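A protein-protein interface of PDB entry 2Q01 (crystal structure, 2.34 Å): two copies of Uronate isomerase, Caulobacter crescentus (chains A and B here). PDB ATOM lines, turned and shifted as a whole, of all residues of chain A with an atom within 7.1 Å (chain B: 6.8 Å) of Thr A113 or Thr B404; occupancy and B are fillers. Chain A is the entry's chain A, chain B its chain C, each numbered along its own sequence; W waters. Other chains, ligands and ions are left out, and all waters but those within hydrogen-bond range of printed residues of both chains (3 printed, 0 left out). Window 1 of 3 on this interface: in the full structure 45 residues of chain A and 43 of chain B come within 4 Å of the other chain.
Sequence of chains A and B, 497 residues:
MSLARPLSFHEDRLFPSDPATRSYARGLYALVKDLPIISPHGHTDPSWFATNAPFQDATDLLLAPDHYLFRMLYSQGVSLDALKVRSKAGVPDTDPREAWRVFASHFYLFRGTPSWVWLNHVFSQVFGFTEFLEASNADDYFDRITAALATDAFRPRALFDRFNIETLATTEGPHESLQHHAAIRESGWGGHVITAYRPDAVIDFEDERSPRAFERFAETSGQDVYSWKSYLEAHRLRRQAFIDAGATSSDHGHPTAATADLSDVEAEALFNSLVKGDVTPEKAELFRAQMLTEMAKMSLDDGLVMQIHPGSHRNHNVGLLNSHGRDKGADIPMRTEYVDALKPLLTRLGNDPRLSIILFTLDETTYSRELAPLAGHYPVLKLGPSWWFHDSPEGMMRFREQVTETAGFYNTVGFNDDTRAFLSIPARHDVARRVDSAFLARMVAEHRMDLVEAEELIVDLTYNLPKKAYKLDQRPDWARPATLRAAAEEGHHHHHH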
ATOM      1  N   LEU A  69      -7.301 -23.226  10.622  1.00  0.00           N
ATOM      2  CA  LEU A  69      -7.781 -24.418   9.925  1.00  0.00           C
ATOM      3  C   LEU A  69      -7.706 -24.299   8.407  1.00  0.00           C
ATOM      4  O   LEU A  69      -7.123 -25.168   7.760  1.00  0.00           O
ATOM      5  CB  LEU A  69      -9.206 -24.790  10.363  1.00  0.00           C
ATOM      6  CG  LEU A  69      -9.466 -25.098  11.840  1.00  0.00           C
ATOM      7  CD1 LEU A  69     -10.931 -25.438  12.044  1.00  0.00           C
ATOM      8  CD2 LEU A  69      -8.585 -26.220  12.353  1.00  0.00           C
ATOM      9  N   MET A  72      -3.998 -24.321   6.625  1.00  0.00           N
ATOM     10  CA  MET A  72      -3.462 -25.658   6.368  1.00  0.00           C
ATOM     11  C   MET A  72      -4.027 -26.316   5.127  1.00  0.00           C
ATOM     12  O   MET A  72      -3.290 -26.950   4.378  1.00  0.00           O
ATOM     13  CB  MET A  72      -3.719 -26.600   7.548  1.00  0.00           C
ATOM     14  CG  MET A  72      -2.608 -26.719   8.595  1.00  0.00           C
ATOM     15  SD  MET A  72      -0.987 -27.355   8.086  1.00  0.00           S
ATOM     16  CE  MET A  72      -1.379 -28.518   6.796  1.00  0.00           C
ATOM     17  N   PHE A 107      -8.437 -33.760   7.840  1.00  0.00           N
ATOM     18  CA  PHE A 107      -8.195 -33.536   9.268  1.00  0.00           C
ATOM     19  C   PHE A 107      -6.868 -34.163   9.736  1.00  0.00           C
ATOM     20  O   PHE A 107      -6.348 -33.821  10.801  1.00  0.00           O
ATOM     21  CB  PHE A 107      -9.399 -34.026  10.099  1.00  0.00           C
ATOM     22  CG  PHE A 107      -9.302 -33.708  11.569  1.00  0.00           C
ATOM     23  CD1 PHE A 107      -9.050 -32.407  12.005  1.00  0.00           C
ATOM     24  CD2 PHE A 107      -9.463 -34.712  12.520  1.00  0.00           C
ATOM     25  CE1 PHE A 107      -8.947 -32.116  13.367  1.00  0.00           C
ATOM     26  CE2 PHE A 107      -9.371 -34.428  13.886  1.00  0.00           C
ATOM     27  CZ  PHE A 107      -9.108 -33.129  14.308  1.00  0.00           C
ATOM     28  N   LEU A 109      -4.074 -33.605   8.384  1.00  0.00           N
ATOM     29  CA  LEU A 109      -3.045 -32.578   8.243  1.00  0.00           C
ATOM     30  C   LEU A 109      -2.666 -31.963   9.588  1.00  0.00           C
ATOM     31  O   LEU A 109      -1.561 -31.450   9.760  1.00  0.00           O
ATOM     32  CB  LEU A 109      -3.507 -31.486   7.277  1.00  0.00           C
ATOM     33  CG  LEU A 109      -3.068 -31.638   5.819  1.00  0.00           C
ATOM     34  CD1 LEU A 109      -2.839 -33.103   5.477  1.00  0.00           C
ATOM     35  CD2 LEU A 109      -4.091 -31.017   4.881  1.00  0.00           C
ATOM     36  N   PHE A 110      -3.594 -32.018  10.538  1.00  0.00           N
ATOM     37  CA  PHE A 110      -3.462 -31.304  11.802  1.00  0.00           C
ATOM     38  C   PHE A 110      -2.787 -32.113  12.900  1.00  0.00           C
ATOM     39  O   PHE A 110      -2.772 -31.703  14.064  1.00  0.00           O
ATOM     40  CB  PHE A 110      -4.830 -30.784  12.254  1.00  0.00           C
ATOM     41  CG  PHE A 110      -5.410 -29.765  11.325  1.00  0.00           C
ATOM     42  CD1 PHE A 110      -6.283 -30.146  10.314  1.00  0.00           C
ATOM     43  CD2 PHE A 110      -5.053 -28.426  11.434  1.00  0.00           C
ATOM     44  CE1 PHE A 110      -6.803 -29.213   9.439  1.00  0.00           C
ATOM     45  CE2 PHE A 110      -5.573 -27.484  10.563  1.00  0.00           C
ATOM     46  CZ  PHE A 110      -6.448 -27.879   9.563  1.00  0.00           C
ATOM     47  N   ARG A 111      -2.221 -33.256  12.516  1.00  0.00           N
ATOM     48  CA  ARG A 111      -1.432 -34.079  13.421  1.00  0.00           C
ATOM     49  C   ARG A 111      -0.184 -33.318  13.856  1.00  0.00           C
ATOM     50  O   ARG A 111       0.562 -32.813  13.019  1.00  0.00           O
ATOM     51  CB  ARG A 111      -1.042 -35.399  12.747  1.00  0.00           C
ATOM     52  CG  ARG A 111      -2.192 -36.373  12.585  1.00  0.00           C
ATOM     53  CD  ARG A 111      -1.793 -37.538  11.701  1.00  0.00           C
ATOM     54  NE  ARG A 111      -2.922 -38.400  11.349  1.00  0.00           N
ATOM     55  CZ  ARG A 111      -2.857 -39.406  10.481  1.00  0.00           C
ATOM     56  NH1 ARG A 111      -3.939 -40.128  10.226  1.00  0.00           N
ATOM     57  NH2 ARG A 111      -1.714 -39.693   9.863  1.00  0.00           N
ATOM     58  N   GLY A 112       0.014 -33.203  15.167  1.00  0.00           N
ATOM     59  CA  GLY A 112       1.178 -32.510  15.716  1.00  0.00           C
ATOM     60  C   GLY A 112       0.995 -31.017  15.921  1.00  0.00           C
ATOM     61  O   GLY A 112       1.846 -30.361  16.531  1.00  0.00           O
ATOM     62  N   THR A 113      -0.115 -30.484  15.412  1.00  0.00           N
ATOM     63  CA  THR A 113      -0.441 -29.063  15.515  1.00  0.00           C
ATOM     64  C   THR A 113      -1.360 -28.842  16.717  1.00  0.00           C
ATOM     65  O   THR A 113      -2.084 -29.756  17.099  1.00  0.00           O
ATOM     66  CB  THR A 113      -1.158 -28.568  14.246  1.00  0.00           C
ATOM     67  OG1 THR A 113      -2.507 -29.047  14.242  1.00  0.00           O
ATOM     68  CG2 THR A 113      -0.438 -29.040  12.982  1.00  0.00           C
ATOM     69  N   PRO A 114      -1.340 -27.632  17.321  1.00  0.00           N
ATOM     70  CA  PRO A 114      -2.260 -27.318  18.429  1.00  0.00           C
ATOM     71  C   PRO A 114      -3.757 -27.403  18.095  1.00  0.00           C
ATOM     72  O   PRO A 114      -4.573 -27.562  19.004  1.00  0.00           O
ATOM     73  CB  PRO A 114      -1.886 -25.881  18.808  1.00  0.00           C
ATOM     74  CG  PRO A 114      -1.131 -25.348  17.646  1.00  0.00           C
ATOM     75  CD  PRO A 114      -0.433 -26.506  17.037  1.00  0.00           C
ATOM     76  N   SER A 115      -4.101 -27.306  16.810  1.00  0.00           N
ATOM     77  CA  SER A 115      -5.481 -27.468  16.344  1.00  0.00           C
ATOM     78  C   SER A 115      -6.029 -28.878  16.590  1.00  0.00           C
ATOM     79  O   SER A 115      -7.240 -29.072  16.616  1.00  0.00           O
ATOM     80  CB  SER A 115      -5.603 -27.112  14.859  1.00  0.00           C
ATOM     81  OG  SER A 115      -5.731 -25.713  14.659  1.00  0.00           O
ATOM     82  N   TRP A 116      -5.127 -29.847  16.752  1.00  0.00           N
ATOM     83  CA  TRP A 116      -5.468 -31.229  17.090  1.00  0.00           C
ATOM     84  C   TRP A 116      -6.023 -31.288  18.505  1.00  0.00           C
ATOM     85  O   TRP A 116      -7.044 -31.921  18.754  1.00  0.00           O
ATOM     86  CB  TRP A 116      -4.211 -32.102  17.000  1.00  0.00           C
ATOM     87  CG  TRP A 116      -4.419 -33.595  17.040  1.00  0.00           C
ATOM     88  CD1 TRP A 116      -4.554 -34.430  15.968  1.00  0.00           C
ATOM     89  CD2 TRP A 116      -4.469 -34.430  18.208  1.00  0.00           C
ATOM     90  NE1 TRP A 116      -4.697 -35.731  16.395  1.00  0.00           N
ATOM     91  CE2 TRP A 116      -4.652 -35.758  17.765  1.00  0.00           C
ATOM     92  CE3 TRP A 116      -4.389 -34.182  19.588  1.00  0.00           C
ATOM     93  CZ2 TRP A 116      -4.757 -36.839  18.652  1.00  0.00           C
ATOM     94  CZ3 TRP A 116      -4.493 -35.254  20.470  1.00  0.00           C
ATOM     95  CH2 TRP A 116      -4.674 -36.568  19.998  1.00  0.00           C
ATOM     96  N   VAL A 117      -5.340 -30.608  19.417  1.00  0.00           N
ATOM     97  CA  VAL A 117      -5.694 -30.606  20.824  1.00  0.00           C
ATOM     98  C   VAL A 117      -6.974 -29.811  21.071  1.00  0.00           C
ATOM     99  O   VAL A 117      -7.875 -30.301  21.753  1.00  0.00           O
ATOM    100  CB  VAL A 117      -4.523 -30.090  21.697  1.00  0.00           C
ATOM    101  CG1 VAL A 117      -4.882 -30.119  23.168  1.00  0.00           C
ATOM    102  CG2 VAL A 117      -3.282 -30.941  21.459  1.00  0.00           C
ATOM    103  N   TRP A 118      -7.060 -28.614  20.487  1.00  0.00           N
ATOM    104  CA  TRP A 118      -8.218 -27.732  20.660  1.00  0.00           C
ATOM    105  C   TRP A 118      -9.513 -28.337  20.132  1.00  0.00           C
ATOM    106  O   TRP A 118     -10.536 -28.298  20.812  1.00  0.00           O
ATOM    107  CB  TRP A 118      -8.001 -26.380  19.975  1.00  0.00           C
ATOM    108  CG  TRP A 118      -6.836 -25.597  20.470  1.00  0.00           C
ATOM    109  CD1 TRP A 118      -6.322 -25.590  21.736  1.00  0.00           C
ATOM    110  CD2 TRP A 118      -6.050 -24.669  19.712  1.00  0.00           C
ATOM    111  NE1 TRP A 118      -5.251 -24.730  21.807  1.00  0.00           N
ATOM    112  CE2 TRP A 118      -5.064 -24.150  20.579  1.00  0.00           C
ATOM    113  CE3 TRP A 118      -6.076 -24.234  18.379  1.00  0.00           C
ATOM    114  CZ2 TRP A 118      -4.115 -23.214  20.159  1.00  0.00           C
ATOM    115  CZ3 TRP A 118      -5.131 -23.305  17.960  1.00  0.00           C
ATOM    116  CH2 TRP A 118      -4.165 -22.806  18.847  1.00  0.00           C
ATOM    117  N   SER A 392       0.729 -22.255  21.697  1.00  0.00           N
ATOM    118  CA  SER A 392       0.798 -23.674  21.435  1.00  0.00           C
ATOM    119  C   SER A 392       1.722 -24.286  22.483  1.00  0.00           C
ATOM    120  O   SER A 392       2.545 -23.562  23.048  1.00  0.00           O
ATOM    121  CB  SER A 392       1.414 -23.862  20.056  1.00  0.00           C
ATOM    122  OG  SER A 392       2.802 -23.565  20.088  1.00  0.00           O
ATOM    123  N   PRO A 393       1.600 -25.606  22.748  1.00  0.00           N
ATOM    124  CA  PRO A 393       2.415 -26.255  23.785  1.00  0.00           C
ATOM    125  C   PRO A 393       3.925 -25.973  23.724  1.00  0.00           C
ATOM    126  O   PRO A 393       4.506 -25.578  24.738  1.00  0.00           O
ATOM    127  CB  PRO A 393       2.130 -27.742  23.568  1.00  0.00           C
ATOM    128  CG  PRO A 393       0.775 -27.769  22.994  1.00  0.00           C
ATOM    129  CD  PRO A 393       0.670 -26.566  22.121  1.00  0.00           C
ATOM    130  N   ALA B 372       7.791 -21.827   8.651  1.00  0.00           N
ATOM    131  CA  ALA B 372       6.555 -22.541   8.987  1.00  0.00           C
ATOM    132  C   ALA B 372       5.246 -21.774   8.680  1.00  0.00           C
ATOM    133  O   ALA B 372       4.308 -22.380   8.153  1.00  0.00           O
ATOM    134  CB  ALA B 372       6.590 -23.079  10.445  1.00  0.00           C
ATOM    135  N   PHE B 399      14.193 -28.535  14.673  1.00  0.00           N
ATOM    136  CA  PHE B 399      13.396 -28.457  13.450  1.00  0.00           C
ATOM    137  C   PHE B 399      11.967 -28.896  13.730  1.00  0.00           C
ATOM    138  O   PHE B 399      11.049 -28.105  13.581  1.00  0.00           O
ATOM    139  CB  PHE B 399      14.008 -29.326  12.345  1.00  0.00           C
ATOM    140  CG  PHE B 399      13.270 -29.257  11.032  1.00  0.00           C
ATOM    141  CD1 PHE B 399      12.468 -30.313  10.611  1.00  0.00           C
ATOM    142  CD2 PHE B 399      13.385 -28.139  10.212  1.00  0.00           C
ATOM    143  CE1 PHE B 399      11.788 -30.253   9.396  1.00  0.00           C
ATOM    144  CE2 PHE B 399      12.708 -28.066   8.997  1.00  0.00           C
ATOM    145  CZ  PHE B 399      11.908 -29.126   8.587  1.00  0.00           C
ATOM    146  N   ARG B 400      11.801 -30.143  14.173  1.00  0.00           N
ATOM    147  CA  ARG B 400      10.483 -30.718  14.476  1.00  0.00           C
ATOM    148  C   ARG B 400       9.697 -29.936  15.532  1.00  0.00           C
ATOM    149  O   ARG B 400       8.499 -29.729  15.376  1.00  0.00           O
ATOM    150  CB  ARG B 400      10.607 -32.191  14.902  1.00  0.00           C
ATOM    151  CG  ARG B 400      11.036 -33.166  13.799  1.00  0.00           C
ATOM    152  CD  ARG B 400      10.028 -33.224  12.660  1.00  0.00           C
ATOM    153  NE  ARG B 400      10.530 -33.970  11.505  1.00  0.00           N
ATOM    154  CZ  ARG B 400      10.027 -33.884  10.275  1.00  0.00           C
ATOM    155  NH1 ARG B 400      10.554 -34.602   9.290  1.00  0.00           N
ATOM    156  NH2 ARG B 400       9.001 -33.077  10.021  1.00  0.00           N
ATOM    157  N   GLU B 401      10.369 -29.504  16.595  1.00  0.00           N
ATOM    158  CA  GLU B 401       9.733 -28.712  17.660  1.00  0.00           C
ATOM    159  C   GLU B 401       9.257 -27.323  17.201  1.00  0.00           C
ATOM    160  O   GLU B 401       8.263 -26.797  17.721  1.00  0.00           O
ATOM    161  CB  GLU B 401      10.679 -28.558  18.853  1.00  0.00           C
ATOM    162  CG  GLU B 401      10.879 -29.817  19.693  1.00  0.00           C
ATOM    163  CD  GLU B 401      12.034 -29.694  20.685  1.00  0.00           C
ATOM    164  OE1 GLU B 401      13.104 -29.168  20.304  1.00  0.00           O
ATOM    165  OE2 GLU B 401      11.878 -30.133  21.846  1.00  0.00           O
ATOM    166  N   GLN B 402       9.954 -26.741  16.225  1.00  0.00           N
ATOM    167  CA  GLN B 402       9.675 -25.368  15.786  1.00  0.00           C
ATOM    168  C   GLN B 402       8.851 -25.249  14.501  1.00  0.00           C
ATOM    169  O   GLN B 402       8.200 -24.229  14.283  1.00  0.00           O
ATOM    170  CB  GLN B 402      10.978 -24.573  15.652  1.00  0.00           C
ATOM    171  CG  GLN B 402      11.613 -24.235  16.990  1.00  0.00           C
ATOM    172  CD  GLN B 402      13.029 -23.713  16.877  1.00  0.00           C
ATOM    173  OE1 GLN B 402      13.818 -23.842  17.813  1.00  0.00           O
ATOM    174  NE2 GLN B 402      13.358 -23.113  15.741  1.00  0.00           N
ATOM    175  N   VAL B 403       8.879 -26.285  13.664  1.00  0.00           N
ATOM    176  CA  VAL B 403       8.224 -26.260  12.355  1.00  0.00           C
ATOM    177  C   VAL B 403       6.797 -26.851  12.365  1.00  0.00           C
ATOM    178  O   VAL B 403       5.890 -26.297  11.741  1.00  0.00           O
ATOM    179  CB  VAL B 403       9.151 -26.904  11.285  1.00  0.00           C
ATOM    180  CG1 VAL B 403       8.384 -27.545  10.130  1.00  0.00           C
ATOM    181  CG2 VAL B 403      10.146 -25.874  10.783  1.00  0.00           C
ATOM    182  N   THR B 404       6.617 -27.939  13.119  1.00  0.00           N
ATOM    183  CA  THR B 404       5.412 -28.791  13.097  1.00  0.00           C
ATOM    184  C   THR B 404       4.129 -28.083  13.520  1.00  0.00           C
ATOM    185  O   THR B 404       3.078 -28.246  12.906  1.00  0.00           O
ATOM    186  CB  THR B 404       5.630 -30.039  13.991  1.00  0.00           C
ATOM    187  OG1 THR B 404       6.786 -30.754  13.530  1.00  0.00           O
ATOM    188  CG2 THR B 404       4.412 -30.965  13.989  1.00  0.00           C
ATOM    189  N   GLU B 405       4.241 -27.290  14.573  1.00  0.00           N
ATOM    190  CA  GLU B 405       3.148 -26.492  15.101  1.00  0.00           C
ATOM    191  C   GLU B 405       2.328 -25.725  14.046  1.00  0.00           C
ATOM    192  O   GLU B 405       1.098 -25.725  14.094  1.00  0.00           O
ATOM    193  CB  GLU B 405       3.745 -25.513  16.098  1.00  0.00           C
ATOM    194  CG  GLU B 405       2.964 -25.367  17.354  1.00  0.00           C
ATOM    195  CD  GLU B 405       3.340 -26.375  18.429  1.00  0.00           C
ATOM    196  OE1 GLU B 405       3.989 -25.955  19.406  1.00  0.00           O
ATOM    197  OE2 GLU B 405       2.977 -27.567  18.315  1.00  0.00           O
ATOM    198  N   THR B 406       3.014 -25.093  13.090  1.00  0.00           N
ATOM    199  CA  THR B 406       2.369 -24.255  12.071  1.00  0.00           C
ATOM    200  C   THR B 406       2.310 -24.913  10.684  1.00  0.00           C
ATOM    201  O   THR B 406       1.306 -24.786   9.978  1.00  0.00           O
ATOM    202  CB  THR B 406       3.073 -22.886  11.969  1.00  0.00           C
ATOM    203  OG1 THR B 406       3.098 -22.266  13.260  1.00  0.00           O
ATOM    204  CG2 THR B 406       2.368 -21.971  10.994  1.00  0.00           C
ATOM    205  N   ALA B 407       3.376 -25.615  10.297  1.00  0.00           N
ATOM    206  CA  ALA B 407       3.448 -26.240   8.969  1.00  0.00           C
ATOM    207  C   ALA B 407       2.838 -27.637   8.920  1.00  0.00           C
ATOM    208  O   ALA B 407       2.289 -28.044   7.896  1.00  0.00           O
ATOM    209  CB  ALA B 407       4.889 -26.290   8.473  1.00  0.00           C
ATOM    210  N   GLY B 408       2.954 -28.376  10.019  1.00  0.00           N
ATOM    211  CA  GLY B 408       2.607 -29.792  10.029  1.00  0.00           C
ATOM    212  C   GLY B 408       3.705 -30.647   9.418  1.00  0.00           C
ATOM    213  O   GLY B 408       4.769 -30.145   9.044  1.00  0.00           O
ATOM    214  N   PHE B 409       3.440 -31.946   9.323  1.00  0.00           N
ATOM    215  CA  PHE B 409       4.388 -32.902   8.759  1.00  0.00           C
ATOM    216  C   PHE B 409       4.275 -32.957   7.243  1.00  0.00           C
ATOM    217  O   PHE B 409       5.233 -33.306   6.545  1.00  0.00           O
ATOM    218  CB  PHE B 409       4.133 -34.303   9.333  1.00  0.00           C
ATOM    219  CG  PHE B 409       4.291 -34.391  10.826  1.00  0.00           C
ATOM    220  CD1 PHE B 409       5.552 -34.559  11.396  1.00  0.00           C
ATOM    221  CD2 PHE B 409       3.180 -34.313  11.666  1.00  0.00           C
ATOM    222  CE1 PHE B 409       5.708 -34.645  12.781  1.00  0.00           C
ATOM    223  CE2 PHE B 409       3.326 -34.399  13.056  1.00  0.00           C
ATOM    224  CZ  PHE B 409       4.591 -34.562  13.612  1.00  0.00           C
ATOM    225  N   THR B 412       6.420 -30.721   5.041  1.00  0.00           N
ATOM    226  CA  THR B 412       7.858 -31.020   5.031  1.00  0.00           C
ATOM    227  C   THR B 412       8.170 -32.088   3.975  1.00  0.00           C
ATOM    228  O   THR B 412       7.258 -32.718   3.438  1.00  0.00           O
ATOM    229  CB  THR B 412       8.389 -31.477   6.413  1.00  0.00           C
ATOM    230  OG1 THR B 412       7.910 -32.795   6.710  1.00  0.00           O
ATOM    231  CG2 THR B 412       7.976 -30.505   7.522  1.00  0.00           C
ATOM    232  N   PHE B 439      11.032 -37.926  18.445  1.00  0.00           N
ATOM    233  CA  PHE B 439      10.133 -36.784  18.462  1.00  0.00           C
ATOM    234  C   PHE B 439       8.686 -37.254  18.522  1.00  0.00           C
ATOM    235  O   PHE B 439       7.916 -36.812  19.381  1.00  0.00           O
ATOM    236  CB  PHE B 439      10.355 -35.878  17.241  1.00  0.00           C
ATOM    237  CG  PHE B 439       9.307 -34.810  17.085  1.00  0.00           C
ATOM    238  CD1 PHE B 439       9.261 -33.728  17.971  1.00  0.00           C
ATOM    239  CD2 PHE B 439       8.351 -34.894  16.069  1.00  0.00           C
ATOM    240  CE1 PHE B 439       8.278 -32.739  17.844  1.00  0.00           C
ATOM    241  CE2 PHE B 439       7.363 -33.911  15.930  1.00  0.00           C
ATOM    242  CZ  PHE B 439       7.328 -32.832  16.820  1.00  0.00           C
ATOM    243  N   MET B 443       5.433 -37.181  21.463  1.00  0.00           N
ATOM    244  CA  MET B 443       4.082 -36.699  21.186  1.00  0.00           C
ATOM    245  C   MET B 443       3.045 -37.698  21.677  1.00  0.00           C
ATOM    246  O   MET B 443       1.990 -37.309  22.165  1.00  0.00           O
ATOM    247  CB  MET B 443       3.884 -36.456  19.688  1.00  0.00           C
ATOM    248  CG  MET B 443       4.880 -35.496  19.043  1.00  0.00           C
ATOM    249  SD  MET B 443       4.725 -33.785  19.584  1.00  0.00           S
ATOM    250  CE  MET B 443       3.234 -33.320  18.711  1.00  0.00           C
ATOM    251  N   ARG B 448      -0.263 -36.091  22.731  1.00  0.00           N
ATOM    252  CA  ARG B 448      -0.467 -35.037  21.741  1.00  0.00           C
ATOM    253  C   ARG B 448      -0.749 -35.646  20.371  1.00  0.00           C
ATOM    254  O   ARG B 448      -1.158 -34.943  19.444  1.00  0.00           O
ATOM    255  CB  ARG B 448       0.748 -34.105  21.685  1.00  0.00           C
ATOM    256  CG  ARG B 448       0.982 -33.319  22.964  1.00  0.00           C
ATOM    257  CD  ARG B 448       1.745 -32.032  22.685  1.00  0.00           C
ATOM    258  NE  ARG B 448       3.185 -32.236  22.567  1.00  0.00           N
ATOM    259  CZ  ARG B 448       4.029 -31.351  22.048  1.00  0.00           C
ATOM    260  NH1 ARG B 448       3.587 -30.192  21.578  1.00  0.00           N
ATOM    261  NH2 ARG B 448       5.323 -31.634  21.980  1.00  0.00           N
HETATM  262  O   HOH W   1       0.554 -32.546  10.520  1.00  0.00           O
HETATM  263  O   HOH W   2       0.755 -31.022   7.476  1.00  0.00           O
HETATM  264  O   HOH W   3      -1.487 -35.286  16.469  1.00  0.00           O
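Water W1 lies within hydrogen-bond range of O of Leu A109 (2.5 Å), O of Arg A111 (2.5 Å) and N of Phe B409 (3.2 Å). Water W3 lies within hydrogen-bond range of the backbone NH (N) of Gly A112 (2.9 Å), the backbone carbonyl oxygen (O) of Arg B448 (3.0 Å) and the indole nitrogen (NE1) of Trp A116 (3.2 Å). Water W2 lies within hydrogen-bond range of O of Leu A109 (3.3 Å), O of Ala B407 (3.4 Å) and N of Phe B409 (3.4 Å).
Among the printed residues, pairs that only touch across the chains: Arg A111 with Phe B409, Trp A116 with Arg B448, Pro A114 with Glu B405, Pro A393 with Arg B448, Gly A112 with Glu B405, Thr A113 with Thr B404, Thr A113 with Glu B405, Gly A112 with Thr B404, Gly A112 with Met B443, Gly A112 with Phe B409 and Met A72 with Thr B406.
Printed residues of chain B within 4 Å of Met A72: Thr B406 and Ala B407. Phe A110 touches none of the printed residues of chain B. Of chain B, only Thr B404 (3.7 Å), Glu B405 (3.5 Å), Phe B409 (3.9 Å) and Met B443 (3.7 Å) come within 4 Å of Gly A112. Thr A113 touches two residues of chain B. Of the printed residues of chain B, Pro A393 touches Arg B448. Of chain A, only Gly A112 and Thr A113 come within 4 Å of Thr B404. The nearest residue of chain A that does not touch Thr B404 is Arg A111 (4.4 Å). The nearest printed residue of chain A that does not touch Met B443 is Thr A113 (5.5 Å).
Hydrophobic or aromatic side chains of chain A within 4 Å of the printed part of chain B: Met A72, Pro A114, Trp A116 and Pro A393. Hydrophobic or aromatic side chains of chain B within 4 Å of the printed part of chain A: Phe B409 and Met B443.
No position is printed for both chains.
OE1 of Glu B405 sits at hydrogen-bond distance from OG of Ser A392 (2.8 Å). SD of Met A72 lies close to O of Ala B407.
The backbone carbonyl oxygen (O) of Arg B400 lies within hydrogen-bond range of the side-chain hydroxyl (OG1) of Thr B404 (2.7 Å). OG1 of Thr A113 lies close to N of Ser A115 (3.5 Å). The backbone carbonyl oxygen (O) of Phe A110 lies within hydrogen-bond range of the side-chain hydroxyl (OG1) of Thr A113, 2.7 Å away. The side-chain hydroxyl (OG1) of Thr B412 lies within hydrogen-bond range of the backbone carbonyl oxygen (O) of Phe B409. O of Met B443 sits at hydrogen-bond distance from N of Arg B448 (2.6 Å).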
